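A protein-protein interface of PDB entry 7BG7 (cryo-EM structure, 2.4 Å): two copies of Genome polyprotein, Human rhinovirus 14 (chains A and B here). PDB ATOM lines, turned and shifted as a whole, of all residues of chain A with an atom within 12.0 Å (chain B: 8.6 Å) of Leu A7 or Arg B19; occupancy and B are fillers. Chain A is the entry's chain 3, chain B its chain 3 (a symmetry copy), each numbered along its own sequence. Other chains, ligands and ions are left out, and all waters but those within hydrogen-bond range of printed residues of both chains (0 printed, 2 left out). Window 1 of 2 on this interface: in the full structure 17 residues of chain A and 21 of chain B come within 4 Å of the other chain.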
ATOM      1  N   LEU A   2      23.371  13.967  11.887  1.00  0.00           N
ATOM      2  CA  LEU A   2      21.942  13.793  11.657  1.00  0.00           C
ATOM      3  C   LEU A   2      21.488  14.760  10.569  1.00  0.00           C
ATOM      4  O   LEU A   2      21.571  15.976  10.770  1.00  0.00           O
ATOM      5  CB  LEU A   2      21.165  14.032  12.947  1.00  0.00           C
ATOM      6  CG  LEU A   2      19.639  14.097  12.812  1.00  0.00           C
ATOM      7  CD1 LEU A   2      19.076  12.749  12.407  1.00  0.00           C
ATOM      8  CD2 LEU A   2      19.000  14.578  14.089  1.00  0.00           C
ATOM      9  N   PRO A   3      20.994  14.285   9.427  1.00  0.00           N
ATOM     10  CA  PRO A   3      20.507  15.208   8.392  1.00  0.00           C
ATOM     11  C   PRO A   3      19.352  16.061   8.894  1.00  0.00           C
ATOM     12  O   PRO A   3      18.352  15.548   9.392  1.00  0.00           O
ATOM     13  CB  PRO A   3      20.068  14.270   7.264  1.00  0.00           C
ATOM     14  CG  PRO A   3      20.793  13.009   7.508  1.00  0.00           C
ATOM     15  CD  PRO A   3      20.883  12.884   8.990  1.00  0.00           C
ATOM     16  N   THR A   4      19.513  17.375   8.780  1.00  0.00           N
ATOM     17  CA  THR A   4      18.520  18.339   9.226  1.00  0.00           C
ATOM     18  C   THR A   4      18.218  19.322   8.104  1.00  0.00           C
ATOM     19  O   THR A   4      18.987  19.473   7.153  1.00  0.00           O
ATOM     20  CB  THR A   4      18.975  19.102  10.487  1.00  0.00           C
ATOM     21  OG1 THR A   4      20.250  19.712  10.258  1.00  0.00           O
ATOM     22  CG2 THR A   4      19.068  18.159  11.677  1.00  0.00           C
ATOM     23  N   THR A   5      17.068  19.978   8.218  1.00  0.00           N
ATOM     24  CA  THR A   5      16.651  21.017   7.283  1.00  0.00           C
ATOM     25  C   THR A   5      16.215  22.233   8.086  1.00  0.00           C
ATOM     26  O   THR A   5      15.186  22.194   8.767  1.00  0.00           O
ATOM     27  CB  THR A   5      15.513  20.534   6.380  1.00  0.00           C
ATOM     28  OG1 THR A   5      15.927  19.368   5.662  1.00  0.00           O
ATOM     29  CG2 THR A   5      15.123  21.617   5.378  1.00  0.00           C
ATOM     30  N   THR A   6      16.998  23.303   8.019  1.00  0.00           N
ATOM     31  CA  THR A   6      16.660  24.520   8.744  1.00  0.00           C
ATOM     32  C   THR A   6      15.431  25.161   8.108  1.00  0.00           C
ATOM     33  O   THR A   6      15.349  25.290   6.886  1.00  0.00           O
ATOM     34  CB  THR A   6      17.835  25.499   8.750  1.00  0.00           C
ATOM     35  OG1 THR A   6      18.030  26.034   7.439  1.00  0.00           O
ATOM     36  CG2 THR A   6      19.110  24.811   9.203  1.00  0.00           C
ATOM     37  N   LEU A   7      14.477  25.540   8.939  1.00  0.00           N
ATOM     38  CA  LEU A   7      13.199  26.097   8.530  1.00  0.00           C
ATOM     39  C   LEU A   7      13.260  27.615   8.466  1.00  0.00           C
ATOM     40  O   LEU A   7      14.189  28.233   8.986  1.00  0.00           O
ATOM     41  CB  LEU A   7      12.110  25.667   9.504  1.00  0.00           C
ATOM     42  CG  LEU A   7      11.638  24.216   9.414  1.00  0.00           C
ATOM     43  CD1 LEU A   7      10.585  23.964  10.464  1.00  0.00           C
ATOM     44  CD2 LEU A   7      11.113  23.855   8.026  1.00  0.00           C
ATOM     45  N   PRO A   8      12.288  28.250   7.813  1.00  0.00           N
ATOM     46  CA  PRO A   8      12.184  29.711   7.894  1.00  0.00           C
ATOM     47  C   PRO A   8      12.034  30.177   9.336  1.00  0.00           C
ATOM     48  O   PRO A   8      11.473  29.483  10.184  1.00  0.00           O
ATOM     49  CB  PRO A   8      10.941  30.031   7.054  1.00  0.00           C
ATOM     50  CG  PRO A   8      10.226  28.748   6.907  1.00  0.00           C
ATOM     51  CD  PRO A   8      11.251  27.677   6.945  1.00  0.00           C
ATOM     52  N   GLY A   9      12.558  31.365   9.610  1.00  0.00           N
ATOM     53  CA  GLY A   9      12.618  31.874  10.956  1.00  0.00           C
ATOM     54  C   GLY A   9      13.882  31.486  11.690  1.00  0.00           C
ATOM     55  O   GLY A   9      14.097  31.955  12.812  1.00  0.00           O
ATOM     56  N   SER A  10      14.728  30.653  11.086  1.00  0.00           N
ATOM     57  CA  SER A  10      16.004  30.308  11.692  1.00  0.00           C
ATOM     58  C   SER A  10      16.866  31.553  11.819  1.00  0.00           C
ATOM     59  O   SER A  10      17.039  32.310  10.862  1.00  0.00           O
ATOM     60  CB  SER A  10      16.723  29.242  10.863  1.00  0.00           C
ATOM     61  OG  SER A  10      16.098  27.980  10.995  1.00  0.00           O
ATOM     62  N   GLY A  11      17.367  31.784  13.024  1.00  0.00           N
ATOM     63  CA  GLY A  11      18.215  32.916  13.287  1.00  0.00           C
ATOM     64  C   GLY A  11      17.455  34.162  13.660  1.00  0.00           C
ATOM     65  O   GLY A  11      18.075  35.212  13.853  1.00  0.00           O
ATOM     66  N   GLN A  12      16.134  34.080  13.761  1.00  0.00           N
ATOM     67  CA  GLN A  12      15.327  35.219  14.153  1.00  0.00           C
ATOM     68  C   GLN A  12      15.362  35.369  15.667  1.00  0.00           C
ATOM     69  O   GLN A  12      15.508  34.391  16.403  1.00  0.00           O
ATOM     70  CB  GLN A  12      13.894  35.032  13.659  1.00  0.00           C
ATOM     71  CG  GLN A  12      13.037  34.170  14.570  1.00  0.00           C
ATOM     72  CD  GLN A  12      11.671  33.889  13.992  1.00  0.00           C
ATOM     73  OE1 GLN A  12      11.374  34.275  12.873  1.00  0.00           O
ATOM     74  NE2 GLN A  12      10.820  33.256  14.771  1.00  0.00           N
ATOM     75  N   PHE A  13      15.241  36.605  16.130  1.00  0.00           N
ATOM     76  CA  PHE A  13      15.075  36.895  17.551  1.00  0.00           C
ATOM     77  C   PHE A  13      13.634  37.334  17.772  1.00  0.00           C
ATOM     78  O   PHE A  13      13.282  38.491  17.542  1.00  0.00           O
ATOM     79  CB  PHE A  13      16.071  37.937  18.054  1.00  0.00           C
ATOM     80  CG  PHE A  13      15.760  38.449  19.439  1.00  0.00           C
ATOM     81  CD1 PHE A  13      15.237  37.604  20.402  1.00  0.00           C
ATOM     82  CD2 PHE A  13      16.008  39.762  19.781  1.00  0.00           C
ATOM     83  CE1 PHE A  13      14.950  38.072  21.673  1.00  0.00           C
ATOM     84  CE2 PHE A  13      15.731  40.227  21.051  1.00  0.00           C
ATOM     85  CZ  PHE A  13      15.200  39.382  21.994  1.00  0.00           C
ATOM     86  N   ASP A  17       9.838  34.027  22.723  1.00  0.00           N
ATOM     87  CA  ASP A  17       9.971  32.619  22.363  1.00  0.00           C
ATOM     88  C   ASP A  17      10.168  31.713  23.580  1.00  0.00           C
ATOM     89  O   ASP A  17       9.573  30.632  23.643  1.00  0.00           O
ATOM     90  CB  ASP A  17      11.101  32.440  21.353  1.00  0.00           C
ATOM     91  CG  ASP A  17      11.184  31.020  20.829  1.00  0.00           C
ATOM     92  OD1 ASP A  17      12.287  30.577  20.455  1.00  0.00           O
ATOM     93  OD2 ASP A  17      10.140  30.335  20.808  1.00  0.00           O
ATOM     94  N   GLY B   9      17.792  22.902   0.574  1.00  0.00           N
ATOM     95  CA  GLY B   9      16.504  23.433   0.943  1.00  0.00           C
ATOM     96  C   GLY B   9      16.491  24.083   2.308  1.00  0.00           C
ATOM     97  O   GLY B   9      15.472  24.671   2.685  1.00  0.00           O
ATOM     98  N   SER B  10      17.593  24.004   3.051  1.00  0.00           N
ATOM     99  CA  SER B  10      17.682  24.683   4.334  1.00  0.00           C
ATOM    100  C   SER B  10      17.579  26.185   4.130  1.00  0.00           C
ATOM    101  O   SER B  10      18.273  26.764   3.291  1.00  0.00           O
ATOM    102  CB  SER B  10      18.994  24.328   5.041  1.00  0.00           C
ATOM    103  OG  SER B  10      18.973  22.999   5.524  1.00  0.00           O
ATOM    104  N   GLY B  11      16.673  26.804   4.871  1.00  0.00           N
ATOM    105  CA  GLY B  11      16.477  28.228   4.796  1.00  0.00           C
ATOM    106  C   GLY B  11      15.497  28.643   3.731  1.00  0.00           C
ATOM    107  O   GLY B  11      15.291  29.844   3.535  1.00  0.00           O
ATOM    108  N   GLN B  12      14.891  27.689   3.034  1.00  0.00           N
ATOM    109  CA  GLN B  12      13.904  27.996   2.017  1.00  0.00           C
ATOM    110  C   GLN B  12      12.561  28.266   2.678  1.00  0.00           C
ATOM    111  O   GLN B  12      12.252  27.726   3.742  1.00  0.00           O
ATOM    112  CB  GLN B  12      13.800  26.836   1.030  1.00  0.00           C
ATOM    113  CG  GLN B  12      12.897  25.709   1.499  1.00  0.00           C
ATOM    114  CD  GLN B  12      12.919  24.519   0.570  1.00  0.00           C
ATOM    115  OE1 GLN B  12      13.664  24.494  -0.395  1.00  0.00           O
ATOM    116  NE2 GLN B  12      12.070  23.549   0.835  1.00  0.00           N
ATOM    117  N   PHE B  13      11.766  29.120   2.050  1.00  0.00           N
ATOM    118  CA  PHE B  13      10.382  29.346   2.455  1.00  0.00           C
ATOM    119  C   PHE B  13       9.479  28.697   1.414  1.00  0.00           C
ATOM    120  O   PHE B  13       9.215  29.274   0.360  1.00  0.00           O
ATOM    121  CB  PHE B  13      10.063  30.826   2.643  1.00  0.00           C
ATOM    122  CG  PHE B  13       8.590  31.111   2.804  1.00  0.00           C
ATOM    123  CD1 PHE B  13       7.773  30.229   3.489  1.00  0.00           C
ATOM    124  CD2 PHE B  13       8.029  32.262   2.290  1.00  0.00           C
ATOM    125  CE1 PHE B  13       6.420  30.487   3.638  1.00  0.00           C
ATOM    126  CE2 PHE B  13       6.684  32.524   2.445  1.00  0.00           C
ATOM    127  CZ  PHE B  13       5.881  31.635   3.116  1.00  0.00           C
ATOM    128  N   LEU B  14       9.024  27.491   1.716  1.00  0.00           N
ATOM    129  CA  LEU B  14       8.051  26.790   0.893  1.00  0.00           C
ATOM    130  C   LEU B  14       6.669  27.091   1.455  1.00  0.00           C
ATOM    131  O   LEU B  14       6.408  26.834   2.632  1.00  0.00           O
ATOM    132  CB  LEU B  14       8.329  25.287   0.902  1.00  0.00           C
ATOM    133  CG  LEU B  14       7.397  24.357   0.122  1.00  0.00           C
ATOM    134  CD1 LEU B  14       7.582  24.507  -1.371  1.00  0.00           C
ATOM    135  CD2 LEU B  14       7.620  22.927   0.553  1.00  0.00           C
ATOM    136  N   THR B  16       3.902  25.816   1.518  1.00  0.00           N
ATOM    137  CA  THR B  16       2.983  24.721   1.802  1.00  0.00           C
ATOM    138  C   THR B  16       3.575  23.733   2.801  1.00  0.00           C
ATOM    139  O   THR B  16       3.147  22.578   2.837  1.00  0.00           O
ATOM    140  CB  THR B  16       2.613  23.959   0.522  1.00  0.00           C
ATOM    141  OG1 THR B  16       3.764  23.257   0.036  1.00  0.00           O
ATOM    142  CG2 THR B  16       2.093  24.890  -0.562  1.00  0.00           C
ATOM    143  N   ASP B  17       4.540  24.158   3.617  1.00  0.00           N
ATOM    144  CA  ASP B  17       5.298  23.196   4.412  1.00  0.00           C
ATOM    145  C   ASP B  17       4.571  22.786   5.694  1.00  0.00           C
ATOM    146  O   ASP B  17       4.573  21.603   6.048  1.00  0.00           O
ATOM    147  CB  ASP B  17       6.688  23.748   4.717  1.00  0.00           C
ATOM    148  CG  ASP B  17       7.572  22.730   5.410  1.00  0.00           C
ATOM    149  OD1 ASP B  17       8.470  23.130   6.175  1.00  0.00           O
ATOM    150  OD2 ASP B  17       7.352  21.518   5.203  1.00  0.00           O
ATOM    151  N   ASP B  18       3.955  23.726   6.414  1.00  0.00           N
ATOM    152  CA  ASP B  18       3.098  23.389   7.557  1.00  0.00           C
ATOM    153  C   ASP B  18       3.873  22.675   8.673  1.00  0.00           C
ATOM    154  O   ASP B  18       3.686  21.491   8.947  1.00  0.00           O
ATOM    155  CB  ASP B  18       1.911  22.540   7.089  1.00  0.00           C
ATOM    156  CG  ASP B  18       1.080  22.013   8.237  1.00  0.00           C
ATOM    157  OD1 ASP B  18       0.510  22.824   8.989  1.00  0.00           O
ATOM    158  OD2 ASP B  18       1.002  20.779   8.385  1.00  0.00           O
ATOM    159  N   ARG B  19       4.740  23.439   9.330  1.00  0.00           N
ATOM    160  CA  ARG B  19       5.507  22.958  10.471  1.00  0.00           C
ATOM    161  C   ARG B  19       5.085  23.717  11.727  1.00  0.00           C
ATOM    162  O   ARG B  19       4.277  24.643  11.676  1.00  0.00           O
ATOM    163  CB  ARG B  19       7.017  23.121  10.243  1.00  0.00           C
ATOM    164  CG  ARG B  19       7.577  22.423   9.009  1.00  0.00           C
ATOM    165  CD  ARG B  19       7.224  20.938   8.934  1.00  0.00           C
ATOM    166  NE  ARG B  19       7.665  20.184  10.103  1.00  0.00           N
ATOM    167  CZ  ARG B  19       7.599  18.859  10.209  1.00  0.00           C
ATOM    168  NH1 ARG B  19       7.115  18.129   9.216  1.00  0.00           N
ATOM    169  NH2 ARG B  19       8.021  18.260  11.310  1.00  0.00           N
ATOM    170  N   GLN B  20       5.630  23.305  12.867  1.00  0.00           N
ATOM    171  CA  GLN B  20       5.402  24.038  14.104  1.00  0.00           C
ATOM    172  C   GLN B  20       6.180  25.344  14.072  1.00  0.00           C
ATOM    173  O   GLN B  20       7.215  25.456  13.412  1.00  0.00           O
ATOM    174  CB  GLN B  20       5.837  23.208  15.309  1.00  0.00           C
ATOM    175  CG  GLN B  20       5.129  21.880  15.464  1.00  0.00           C
ATOM    176  CD  GLN B  20       5.696  21.047  16.601  1.00  0.00           C
ATOM    177  OE1 GLN B  20       5.790  21.502  17.736  1.00  0.00           O
ATOM    178  NE2 GLN B  20       6.087  19.818  16.291  1.00  0.00           N
ATOM    179  N   SER B  21       5.673  26.342  14.787  1.00  0.00           N
ATOM    180  CA  SER B  21       6.336  27.637  14.850  1.00  0.00           C
ATOM    181  C   SER B  21       6.081  28.271  16.205  1.00  0.00           C
ATOM    182  O   SER B  21       5.041  28.017  16.820  1.00  0.00           O
ATOM    183  CB  SER B  21       5.862  28.578  13.730  1.00  0.00           C
ATOM    184  OG  SER B  21       4.502  28.930  13.878  1.00  0.00           O
ATOM    185  N   PRO B  22       7.004  29.088  16.698  1.00  0.00           N
ATOM    186  CA  PRO B  22       6.805  29.707  18.010  1.00  0.00           C
ATOM    187  C   PRO B  22       5.648  30.692  17.992  1.00  0.00           C
ATOM    188  O   PRO B  22       5.387  31.374  17.000  1.00  0.00           O
ATOM    189  CB  PRO B  22       8.136  30.417  18.273  1.00  0.00           C
ATOM    190  CG  PRO B  22       8.697  30.653  16.922  1.00  0.00           C
ATOM    191  CD  PRO B  22       8.273  29.505  16.083  1.00  0.00           C
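The side-chain hydroxyl (OG) of Ser A10 sits at hydrogen-bond distance from the backbone carbonyl oxygen (O) of Leu A7, at 2.8 Å.
6 positions are printed for both chains.
The side-chain hydroxyl (OG) of Ser B10 is in hydrogen-bond range of the backbone NH (N) of Thr A6, 3.2 Å away. N of Gly B11 lies within hydrogen-bond range of O of Thr A6.
Of the 13 printed residues of chain B, 6 touch a printed residue of chain A. Printed residues of chain B that touch a printed residue of chain A: Ser B10, Gly B11, Gln B12, Asp B17, Arg B19 and Pro B22. Hydrophobic or aromatic side chains of chain B within 4 Å of the printed part of chain A: Pro B22. Printed residues of chain A that touch a printed residue of chain B: Thr A4, Thr A5, Thr A6, Leu A7, Pro A8, Gln A12 and Asp A17. Among the printed residues, 9 pairs touch across the chains.
Among the printed residues, pairs that only touch across the chains: Thr A4 with Ser B10 (3.9 Å), Thr A5 with Ser B10 (3.5 Å), Leu A7 with Asp B17 (3.3 Å), Leu A7 with Arg B19 (3.7 Å), Pro A8 with Gln B12 (3.4 Å), Gln A12 with Pro B22 (3.99 Å) and Asp A17 with Pro B22 (3.2 Å).
Of chain B, only Asp B17 (3.3 Å) and Arg B19 (3.7 Å) come within 4 Å of Leu A7. Of chain A, only Leu A7 (3.7 Å) comes within 4 Å of Arg B19. Of chain B, only Gln B12 comes within 4 Å of Pro A8. Of chain A, only Thr A6 comes within 4 Å of Gly B11. Asp B17 touches one residue of chain A. No residue of chain A comes within 4 Å of Asp B18. No residue of chain A comes within 4 Å of Gln B20. No residue of chain A comes within 4 Å of Ser B21. Of the printed residues of chain B, Thr A6 touches Ser B10 (3.1 Å) and Gly B11 (2.8 Å). Of the printed residues of chain A, Pro B22 touches Gln A12 (3.99 Å) and Asp A17 (3.2 Å). Of the printed residues of chain B, Thr A5 touches Ser B10 (3.5 Å). Phe B13 touches none of the printed residues of chain A. Gly A11 touches none of the printed residues of chain B. The nearest residue of chain B that does not touch Leu A7 is Gln B20 (4.7 Å).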
